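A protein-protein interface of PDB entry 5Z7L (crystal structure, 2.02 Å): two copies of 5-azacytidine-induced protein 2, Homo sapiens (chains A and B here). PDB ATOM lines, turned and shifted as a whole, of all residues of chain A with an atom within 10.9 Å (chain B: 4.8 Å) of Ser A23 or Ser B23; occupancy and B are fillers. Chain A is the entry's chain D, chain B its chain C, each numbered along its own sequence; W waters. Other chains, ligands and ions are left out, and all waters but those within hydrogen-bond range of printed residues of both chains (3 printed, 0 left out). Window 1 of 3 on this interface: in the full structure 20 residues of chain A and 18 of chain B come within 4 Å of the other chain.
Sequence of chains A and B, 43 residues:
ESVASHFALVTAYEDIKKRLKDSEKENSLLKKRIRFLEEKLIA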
ATOM      1  N   ASP A  15     -34.191  20.923   7.367  1.00  0.00           N
ATOM      2  CA  ASP A  15     -34.114  22.258   7.946  1.00  0.00           C
ATOM      3  C   ASP A  15     -32.688  22.639   8.315  1.00  0.00           C
ATOM      4  O   ASP A  15     -32.308  23.811   8.204  1.00  0.00           O
ATOM      5  CB  ASP A  15     -35.008  22.372   9.178  1.00  0.00           C
ATOM      6  CG  ASP A  15     -35.408  23.804   9.453  1.00  0.00           C
ATOM      7  OD1 ASP A  15     -36.174  24.371   8.633  1.00  0.00           O
ATOM      8  OD2 ASP A  15     -34.956  24.354  10.477  1.00  0.00           O
ATOM      9  N   ILE A  16     -31.894  21.680   8.788  1.00  0.00           N
ATOM     10  CA  ILE A  16     -30.517  22.004   9.148  1.00  0.00           C
ATOM     11  C   ILE A  16     -29.699  22.339   7.899  1.00  0.00           C
ATOM     12  O   ILE A  16     -28.898  23.282   7.896  1.00  0.00           O
ATOM     13  CB  ILE A  16     -29.918  20.849   9.973  1.00  0.00           C
ATOM     14  CG1 ILE A  16     -30.509  20.901  11.386  1.00  0.00           C
ATOM     15  CG2 ILE A  16     -28.408  20.956  10.061  1.00  0.00           C
ATOM     16  CD1 ILE A  16     -30.302  19.639  12.181  1.00  0.00           C
ATOM     17  N   LYS A  17     -29.921  21.616   6.802  1.00  0.00           N
ATOM     18  CA  LYS A  17     -29.221  21.980   5.577  1.00  0.00           C
ATOM     19  C   LYS A  17     -29.653  23.356   5.070  1.00  0.00           C
ATOM     20  O   LYS A  17     -28.826  24.085   4.519  1.00  0.00           O
ATOM     21  CB  LYS A  17     -29.403  20.884   4.521  1.00  0.00           C
ATOM     22  CG  LYS A  17     -30.440  21.125   3.467  1.00  0.00           C
ATOM     23  CD  LYS A  17     -30.577  19.872   2.566  1.00  0.00           C
ATOM     24  CE  LYS A  17     -31.695  20.076   1.560  1.00  0.00           C
ATOM     25  NZ  LYS A  17     -31.858  18.897   0.668  1.00  0.00           N
ATOM     26  N   LYS A  18     -30.911  23.764   5.295  1.00  0.00           N
ATOM     27  CA  LYS A  18     -31.286  25.134   4.930  1.00  0.00           C
ATOM     28  C   LYS A  18     -30.608  26.151   5.849  1.00  0.00           C
ATOM     29  O   LYS A  18     -30.149  27.207   5.397  1.00  0.00           O
ATOM     30  CB  LYS A  18     -32.806  25.309   4.965  1.00  0.00           C
ATOM     31  CG  LYS A  18     -33.268  26.773   5.021  1.00  0.00           C
ATOM     32  CD  LYS A  18     -34.703  26.943   5.570  1.00  0.00           C
ATOM     33  CE  LYS A  18     -34.755  26.931   7.112  1.00  0.00           C
ATOM     34  NZ  LYS A  18     -34.771  28.299   7.736  1.00  0.00           N
ATOM     35  N   ARG A  19     -30.526  25.852   7.140  1.00  0.00           N
ATOM     36  CA  ARG A  19     -29.814  26.744   8.047  1.00  0.00           C
ATOM     37  C   ARG A  19     -28.325  26.806   7.728  1.00  0.00           C
ATOM     38  O   ARG A  19     -27.708  27.862   7.889  1.00  0.00           O
ATOM     39  CB  ARG A  19     -30.044  26.302   9.486  1.00  0.00           C
ATOM     40  CG  ARG A  19     -31.504  26.405   9.872  1.00  0.00           C
ATOM     41  CD  ARG A  19     -31.739  25.835  11.246  1.00  0.00           C
ATOM     42  NE  ARG A  19     -30.871  26.471  12.227  1.00  0.00           N
ATOM     43  CZ  ARG A  19     -30.876  26.170  13.519  1.00  0.00           C
ATOM     44  NH1 ARG A  19     -31.699  25.229  13.971  1.00  0.00           N
ATOM     45  NH2 ARG A  19     -30.054  26.804  14.351  1.00  0.00           N
ATOM     46  N   LEU A  20     -27.731  25.697   7.278  1.00  0.00           N
ATOM     47  CA  LEU A  20     -26.326  25.738   6.888  1.00  0.00           C
ATOM     48  C   LEU A  20     -26.125  26.678   5.705  1.00  0.00           C
ATOM     49  O   LEU A  20     -25.244  27.536   5.730  1.00  0.00           O
ATOM     50  CB  LEU A  20     -25.818  24.327   6.555  1.00  0.00           C
ATOM     51  CG  LEU A  20     -24.397  24.269   5.968  1.00  0.00           C
ATOM     52  CD1 LEU A  20     -23.361  24.871   6.928  1.00  0.00           C
ATOM     53  CD2 LEU A  20     -24.000  22.844   5.565  1.00  0.00           C
ATOM     54  N   LYS A  21     -26.963  26.549   4.671  1.00  0.00           N
ATOM     55  CA  LYS A  21     -26.877  27.420   3.496  1.00  0.00           C
ATOM     56  C   LYS A  21     -27.013  28.895   3.879  1.00  0.00           C
ATOM     57  O   LYS A  21     -26.228  29.741   3.430  1.00  0.00           O
ATOM     58  CB  LYS A  21     -27.953  27.007   2.488  1.00  0.00           C
ATOM     59  CG  LYS A  21     -27.932  27.686   1.150  1.00  0.00           C
ATOM     60  CD  LYS A  21     -29.302  27.542   0.500  1.00  0.00           C
ATOM     61  CE  LYS A  21     -29.399  28.274  -0.835  1.00  0.00           C
ATOM     62  NZ  LYS A  21     -29.086  27.397  -1.998  1.00  0.00           N
ATOM     63  N   ASP A  22     -28.002  29.219   4.722  1.00  0.00           N
ATOM     64  CA  ASP A  22     -28.183  30.600   5.160  1.00  0.00           C
ATOM     65  C   ASP A  22     -27.004  31.093   5.990  1.00  0.00           C
ATOM     66  O   ASP A  22     -26.579  32.246   5.848  1.00  0.00           O
ATOM     67  CB  ASP A  22     -29.480  30.743   5.964  1.00  0.00           C
ATOM     68  CG  ASP A  22     -30.720  30.617   5.091  1.00  0.00           C
ATOM     69  OD1 ASP A  22     -30.573  30.678   3.847  1.00  0.00           O
ATOM     70  OD2 ASP A  22     -31.830  30.463   5.650  1.00  0.00           O
ATOM     71  N   SER A  23     -26.495  30.250   6.895  1.00  0.00           N
ATOM     72  CA  SER A  23     -25.345  30.638   7.695  1.00  0.00           C
ATOM     73  C   SER A  23     -24.128  30.919   6.811  1.00  0.00           C
ATOM     74  O   SER A  23     -23.367  31.863   7.066  1.00  0.00           O
ATOM     75  CB  SER A  23     -25.041  29.545   8.722  1.00  0.00           C
ATOM     76  OG  SER A  23     -23.946  29.916   9.536  1.00  0.00           O
ATOM     77  N   GLU A  24     -23.927  30.118   5.761  1.00  0.00           N
ATOM     78  CA  GLU A  24     -22.804  30.371   4.858  1.00  0.00           C
ATOM     79  C   GLU A  24     -23.034  31.634   4.028  1.00  0.00           C
ATOM     80  O   GLU A  24     -22.103  32.416   3.794  1.00  0.00           O
ATOM     81  CB  GLU A  24     -22.568  29.146   3.963  1.00  0.00           C
ATOM     82  CG  GLU A  24     -21.968  27.965   4.711  1.00  0.00           C
ATOM     83  CD  GLU A  24     -20.587  28.281   5.293  1.00  0.00           C
ATOM     84  OE1 GLU A  24     -19.598  28.299   4.523  1.00  0.00           O
ATOM     85  OE2 GLU A  24     -20.495  28.550   6.513  1.00  0.00           O
ATOM     86  N   LYS A  25     -24.274  31.872   3.597  1.00  0.00           N
ATOM     87  CA  LYS A  25     -24.565  33.122   2.907  1.00  0.00           C
ATOM     88  C   LYS A  25     -24.257  34.313   3.809  1.00  0.00           C
ATOM     89  O   LYS A  25     -23.686  35.314   3.356  1.00  0.00           O
ATOM     90  CB  LYS A  25     -26.027  33.148   2.443  1.00  0.00           C
ATOM     91  CG  LYS A  25     -26.507  34.460   1.802  1.00  0.00           C
ATOM     92  CD  LYS A  25     -25.410  35.147   0.941  1.00  0.00           C
ATOM     93  CE  LYS A  25     -25.903  35.633  -0.431  1.00  0.00           C
ATOM     94  NZ  LYS A  25     -26.718  36.866  -0.319  1.00  0.00           N
ATOM     95  N   GLU A  26     -24.640  34.230   5.088  1.00  0.00           N
ATOM     96  CA  GLU A  26     -24.390  35.361   5.964  1.00  0.00           C
ATOM     97  C   GLU A  26     -22.897  35.547   6.186  1.00  0.00           C
ATOM     98  O   GLU A  26     -22.402  36.676   6.160  1.00  0.00           O
ATOM     99  CB  GLU A  26     -25.121  35.210   7.298  1.00  0.00           C
ATOM    100  CG  GLU A  26     -24.890  36.441   8.172  1.00  0.00           C
ATOM    101  CD  GLU A  26     -25.675  36.429   9.471  1.00  0.00           C
ATOM    102  OE1 GLU A  26     -26.922  36.393   9.412  1.00  0.00           O
ATOM    103  OE2 GLU A  26     -25.040  36.462  10.549  1.00  0.00           O
ATOM    104  N   ASN A  27     -22.159  34.453   6.373  1.00  0.00           N
ATOM    105  CA  ASN A  27     -20.710  34.568   6.516  1.00  0.00           C
ATOM    106  C   ASN A  27     -20.082  35.239   5.296  1.00  0.00           C
ATOM    107  O   ASN A  27     -19.152  36.039   5.430  1.00  0.00           O
ATOM    108  CB  ASN A  27     -20.089  33.188   6.767  1.00  0.00           C
ATOM    109  CG  ASN A  27     -20.467  32.623   8.130  1.00  0.00           C
ATOM    110  OD1 ASN A  27     -21.088  33.313   8.949  1.00  0.00           O
ATOM    111  ND2 ASN A  27     -20.132  31.354   8.370  1.00  0.00           N
ATOM    112  N   SER A  28     -20.580  34.944   4.097  1.00  0.00           N
ATOM    113  CA  SER A  28     -20.043  35.608   2.913  1.00  0.00           C
ATOM    114  C   SER A  28     -20.288  37.108   2.967  1.00  0.00           C
ATOM    115  O   SER A  28     -19.418  37.891   2.596  1.00  0.00           O
ATOM    116  CB  SER A  28     -20.647  35.018   1.644  1.00  0.00           C
ATOM    117  OG  SER A  28     -20.315  35.817   0.527  1.00  0.00           O
ATOM    118  N   LEU A  29     -21.464  37.520   3.450  1.00  0.00           N
ATOM    119  CA  LEU A  29     -21.765  38.944   3.597  1.00  0.00           C
ATOM    120  C   LEU A  29     -20.930  39.585   4.700  1.00  0.00           C
ATOM    121  O   LEU A  29     -20.527  40.755   4.594  1.00  0.00           O
ATOM    122  CB  LEU A  29     -23.252  39.128   3.889  1.00  0.00           C
ATOM    123  CG  LEU A  29     -24.190  38.645   2.775  1.00  0.00           C
ATOM    124  CD1 LEU A  29     -25.648  38.633   3.263  1.00  0.00           C
ATOM    125  CD2 LEU A  29     -24.026  39.524   1.527  1.00  0.00           C
ATOM    126  N   LEU A  30     -20.671  38.855   5.776  1.00  0.00           N
ATOM    127  CA  LEU A  30     -19.812  39.401   6.822  1.00  0.00           C
ATOM    128  C   LEU A  30     -18.384  39.594   6.313  1.00  0.00           C
ATOM    129  O   LEU A  30     -17.733  40.584   6.655  1.00  0.00           O
ATOM    130  CB  LEU A  30     -19.832  38.493   8.046  1.00  0.00           C
ATOM    131  CG  LEU A  30     -21.206  38.280   8.670  1.00  0.00           C
ATOM    132  CD1 LEU A  30     -21.117  37.180   9.738  1.00  0.00           C
ATOM    133  CD2 LEU A  30     -21.747  39.595   9.236  1.00  0.00           C
ATOM    134  N   LYS A  31     -17.877  38.669   5.493  1.00  0.00           N
ATOM    135  CA  LYS A  31     -16.551  38.864   4.905  1.00  0.00           C
ATOM    136  C   LYS A  31     -16.505  40.097   4.006  1.00  0.00           C
ATOM    137  O   LYS A  31     -15.494  40.809   3.973  1.00  0.00           O
ATOM    138  CB  LYS A  31     -16.122  37.624   4.117  1.00  0.00           C
ATOM    139  CG  LYS A  31     -15.836  36.420   4.997  1.00  0.00           C
ATOM    140  CD  LYS A  31     -15.645  35.153   4.139  1.00  0.00           C
ATOM    141  CE  LYS A  31     -15.122  34.012   4.971  1.00  0.00           C
ATOM    142  NZ  LYS A  31     -15.167  32.696   4.250  1.00  0.00           N
ATOM    143  N   ARG B  19     -21.046  20.728  10.187  1.00  0.00           N
ATOM    144  CA  ARG B  19     -20.780  21.859   9.298  1.00  0.00           C
ATOM    145  C   ARG B  19     -21.518  23.115   9.747  1.00  0.00           C
ATOM    146  O   ARG B  19     -20.977  24.222   9.658  1.00  0.00           O
ATOM    147  CB  ARG B  19     -21.167  21.493   7.870  1.00  0.00           C
ATOM    148  CG  ARG B  19     -20.209  20.464   7.280  1.00  0.00           C
ATOM    149  CD  ARG B  19     -20.703  19.964   5.913  1.00  0.00           C
ATOM    150  NE  ARG B  19     -20.682  21.018   4.903  1.00  0.00           N
ATOM    151  CZ  ARG B  19     -20.993  20.829   3.621  1.00  0.00           C
ATOM    152  NH1 ARG B  19     -21.339  19.625   3.194  1.00  0.00           N
ATOM    153  NH2 ARG B  19     -20.967  21.843   2.766  1.00  0.00           N
ATOM    154  N   LEU B  20     -22.766  22.969  10.198  1.00  0.00           N
ATOM    155  CA  LEU B  20     -23.501  24.128  10.701  1.00  0.00           C
ATOM    156  C   LEU B  20     -22.812  24.699  11.938  1.00  0.00           C
ATOM    157  O   LEU B  20     -22.673  25.921  12.072  1.00  0.00           O
ATOM    158  CB  LEU B  20     -24.957  23.749  11.001  1.00  0.00           C
ATOM    159  CG  LEU B  20     -25.821  24.864  11.608  1.00  0.00           C
ATOM    160  CD1 LEU B  20     -25.805  26.091  10.708  1.00  0.00           C
ATOM    161  CD2 LEU B  20     -27.251  24.409  11.871  1.00  0.00           C
ATOM    162  N   LYS B  21     -22.315  23.823  12.816  1.00  0.00           N
ATOM    163  CA  LYS B  21     -21.578  24.261  14.002  1.00  0.00           C
ATOM    164  C   LYS B  21     -20.322  25.029  13.622  1.00  0.00           C
ATOM    165  O   LYS B  21     -20.030  26.085  14.198  1.00  0.00           O
ATOM    166  CB  LYS B  21     -21.208  23.055  14.863  1.00  0.00           C
ATOM    167  CG  LYS B  21     -20.730  23.410  16.261  1.00  0.00           C
ATOM    168  CD  LYS B  21     -20.078  22.194  16.927  1.00  0.00           C
ATOM    169  CE  LYS B  21     -19.945  22.372  18.433  1.00  0.00           C
ATOM    170  NZ  LYS B  21     -21.141  21.875  19.174  1.00  0.00           N
ATOM    171  N   ASP B  22     -19.539  24.485  12.687  1.00  0.00           N
ATOM    172  CA  ASP B  22     -18.371  25.205  12.195  1.00  0.00           C
ATOM    173  C   ASP B  22     -18.770  26.531  11.577  1.00  0.00           C
ATOM    174  O   ASP B  22     -18.066  27.532  11.730  1.00  0.00           O
ATOM    175  CB  ASP B  22     -17.613  24.369  11.158  1.00  0.00           C
ATOM    176  CG  ASP B  22     -16.922  23.155  11.766  1.00  0.00           C
ATOM    177  OD1 ASP B  22     -16.714  23.116  13.003  1.00  0.00           O
ATOM    178  OD2 ASP B  22     -16.584  22.240  10.988  1.00  0.00           O
ATOM    179  N   SER B  23     -19.894  26.552  10.859  1.00  0.00           N
ATOM    180  CA  SER B  23     -20.352  27.785  10.223  1.00  0.00           C
ATOM    181  C   SER B  23     -20.780  28.827  11.258  1.00  0.00           C
ATOM    182  O   SER B  23     -20.532  30.026  11.075  1.00  0.00           O
ATOM    183  CB  SER B  23     -21.500  27.464   9.256  1.00  0.00           C
ATOM    184  OG  SER B  23     -21.867  28.598   8.496  1.00  0.00           O
ATOM    185  N   GLU B  24     -21.443  28.402  12.344  1.00  0.00           N
ATOM    186  CA  GLU B  24     -21.792  29.364  13.390  1.00  0.00           C
ATOM    187  C   GLU B  24     -20.542  29.893  14.088  1.00  0.00           C
ATOM    188  O   GLU B  24     -20.505  31.057  14.495  1.00  0.00           O
ATOM    189  CB  GLU B  24     -22.735  28.728  14.432  1.00  0.00           C
ATOM    190  CG  GLU B  24     -24.027  28.116  13.880  1.00  0.00           C
ATOM    191  CD  GLU B  24     -24.820  27.317  14.935  1.00  0.00           C
ATOM    192  OE1 GLU B  24     -24.226  26.841  15.938  1.00  0.00           O
ATOM    193  OE2 GLU B  24     -26.049  27.169  14.762  1.00  0.00           O
ATOM    194  N   LYS B  25     -19.521  29.049  14.268  1.00  0.00           N
ATOM    195  CA  LYS B  25     -18.319  29.541  14.931  1.00  0.00           C
ATOM    196  C   LYS B  25     -17.600  30.552  14.049  1.00  0.00           C
ATOM    197  O   LYS B  25     -17.167  31.600  14.534  1.00  0.00           O
ATOM    198  CB  LYS B  25     -17.408  28.378  15.335  1.00  0.00           C
ATOM    199  CG  LYS B  25     -18.103  27.440  16.332  1.00  0.00           C
ATOM    200  CD  LYS B  25     -17.402  26.085  16.497  1.00  0.00           C
ATOM    201  CE  LYS B  25     -17.903  25.316  17.731  1.00  0.00           C
ATOM    202  NZ  LYS B  25     -18.689  26.128  18.716  1.00  0.00           N
ATOM    203  N   GLU B  26     -17.514  30.291  12.742  1.00  0.00           N
ATOM    204  CA  GLU B  26     -16.958  31.305  11.853  1.00  0.00           C
ATOM    205  C   GLU B  26     -17.816  32.566  11.848  1.00  0.00           C
ATOM    206  O   GLU B  26     -17.286  33.682  11.906  1.00  0.00           O
ATOM    207  CB  GLU B  26     -16.807  30.753  10.438  1.00  0.00           C
ATOM    208  CG  GLU B  26     -15.816  31.554   9.591  1.00  0.00           C
ATOM    209  CD  GLU B  26     -15.985  31.320   8.101  1.00  0.00           C
ATOM    210  OE1 GLU B  26     -16.835  30.486   7.717  1.00  0.00           O
ATOM    211  OE2 GLU B  26     -15.262  31.973   7.317  1.00  0.00           O
ATOM    212  N   ASN B  27     -19.141  32.410  11.799  1.00  0.00           N
ATOM    213  CA  ASN B  27     -20.039  33.559  11.930  1.00  0.00           C
ATOM    214  C   ASN B  27     -19.688  34.381  13.161  1.00  0.00           C
ATOM    215  O   ASN B  27     -19.637  35.618  13.111  1.00  0.00           O
ATOM    216  CB  ASN B  27     -21.491  33.071  12.005  1.00  0.00           C
ATOM    217  CG  ASN B  27     -22.518  34.196  11.872  1.00  0.00           C
ATOM    218  OD1 ASN B  27     -23.076  34.669  12.875  1.00  0.00           O
ATOM    219  ND2 ASN B  27     -22.815  34.592  10.631  1.00  0.00           N
HETATM  220  O   HOH W   1     -27.651  25.348  15.691  1.00  0.00           O
HETATM  221  O   HOH W   2     -27.635  28.846  13.085  1.00  0.00           O
HETATM  222  O   HOH W   3     -17.706  27.558   7.766  1.00  0.00           O
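Printed residues of chain B within 4 Å of Arg A19: Leu B20 (3.8 Å).
Printed residues of chain B within 4 Å of Leu A20: Arg B19 (3.7 Å), Leu B20 (3.8 Å) and Ser B23 (3.95 Å).
Ser A23 touches just one residue of chain B: Ser B23 (2.7 Å).
Printed residues of chain B within 4 Å of Glu A24: Ser B23.
Of the printed residues of chain B, Glu A26 touches Asn B27.
Of the printed residues of chain B, Asn A27 touches Ser B23, Glu B26 and Asn B27.
Leu B20 touches just these residues of chain A: Arg A19 (3.8 Å) and Leu A20 (3.8 Å).
No residue of chain A comes within 4 Å of Asp B22.
No residue of chain A comes within 4 Å of Glu B24.
Glu B26 touches two residues of chain A.
Of chain A, only Glu A26, Asn A27 and Leu A30 come within 4 Å of Asn B27.
The nearest residue of chain A that does not touch Ser B23 is Arg A19 (5.9 Å).
The nearest printed residue of chain A that does not touch Arg B19 is Glu A24 (5.4 Å).
O of Arg A19 touches CD1 of Leu B20, 3.8 Å away.
O of Arg B19 touches CD1 of Leu A20 (3.7 Å).
Leu A20 touches Leu B20.
CD1 of Leu A20 touches CB of Ser B23 (3.95 Å).
CD1 of Leu A30 touches ND2 of Asn B27, 3.2 Å away.
Water W1 bridges the side-chain carboxylate (OE2) of Glu B24 and the guanidinium group (NH2) of Arg A19.
Water W2 bridges OE2 of Glu B24 and NH2 of Arg A19.
Water W3 lies within hydrogen-bond range of OE1 of Glu B26 (3.1 Å) and OE2 of Glu A24 (3.2 Å).
The side-chain amide nitrogen of Asn B27 sits at hydrogen-bond distance from the side-chain amide oxygen of Asn A27, at 2.7 Å.
OE2 of Glu A24 sits at hydrogen-bond distance from OG of Ser B23, at 2.4 Å.
OG of Ser B23 sits at hydrogen-bond distance from OG of Ser A23 (2.7 Å).
The side-chain carboxylate of Glu B26 sits at hydrogen-bond distance from the side-chain amide nitrogen of Asn A27 (3.5 Å).
The side-chain carboxylate of Glu A26 is in hydrogen-bond range of the side-chain amide nitrogen of Asn B27, 2.9 Å away.
NZ of Lys A31 is in salt-bridge range of OE2 of Glu B26.
O of Ser B23 is in hydrogen-bond range of ND2 of Asn A27, at 3.0 Å.
O of Ser A23 sits close to OD1 of Asn A27.
The side-chain carboxylate of Glu A24 is in hydrogen-bond range of the side-chain amide nitrogen of Asn A27, at 3.4 Å.
Hydrophobic or aromatic side chains of chain B that line the printed part of chain A: Leu B20.
Of the 17 printed residues of chain A, 8 touch a printed residue of chain B.
Printed residues of chain A that touch a printed residue of chain B: Arg A19, Leu A20, Ser A23, Glu A24, Glu A26, Asn A27, Leu A30 and Lys A31.
Hydrophobic or aromatic side chains of chain A that line the printed part of chain B: Leu A20 and Leu A30.
Along chain A the printed residues that touch a printed residue of chain B span positions 19 to 31.
Among the printed residues, 12 pairs touch across the chains.
Among the printed residues, Asp or Glu carboxylates within 4 Å of a Lys or Arg side-chain nitrogen of the other chain: Lys A31 with Glu B26 (3.2 Å).
Leu A20 touches Ser B23, but with the chains exchanged Ser A23 does not touch Leu B20 (4.1 Å).
Ser B23 touches its own counterpart, Ser A23.
Glu A24 touches Ser B23, but with the chains exchanged Ser A23 does not touch Glu B24 (4.1 Å).
Glu A26 touches Asn B27, and with the chains exchanged Asn A27 touches Glu B26.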
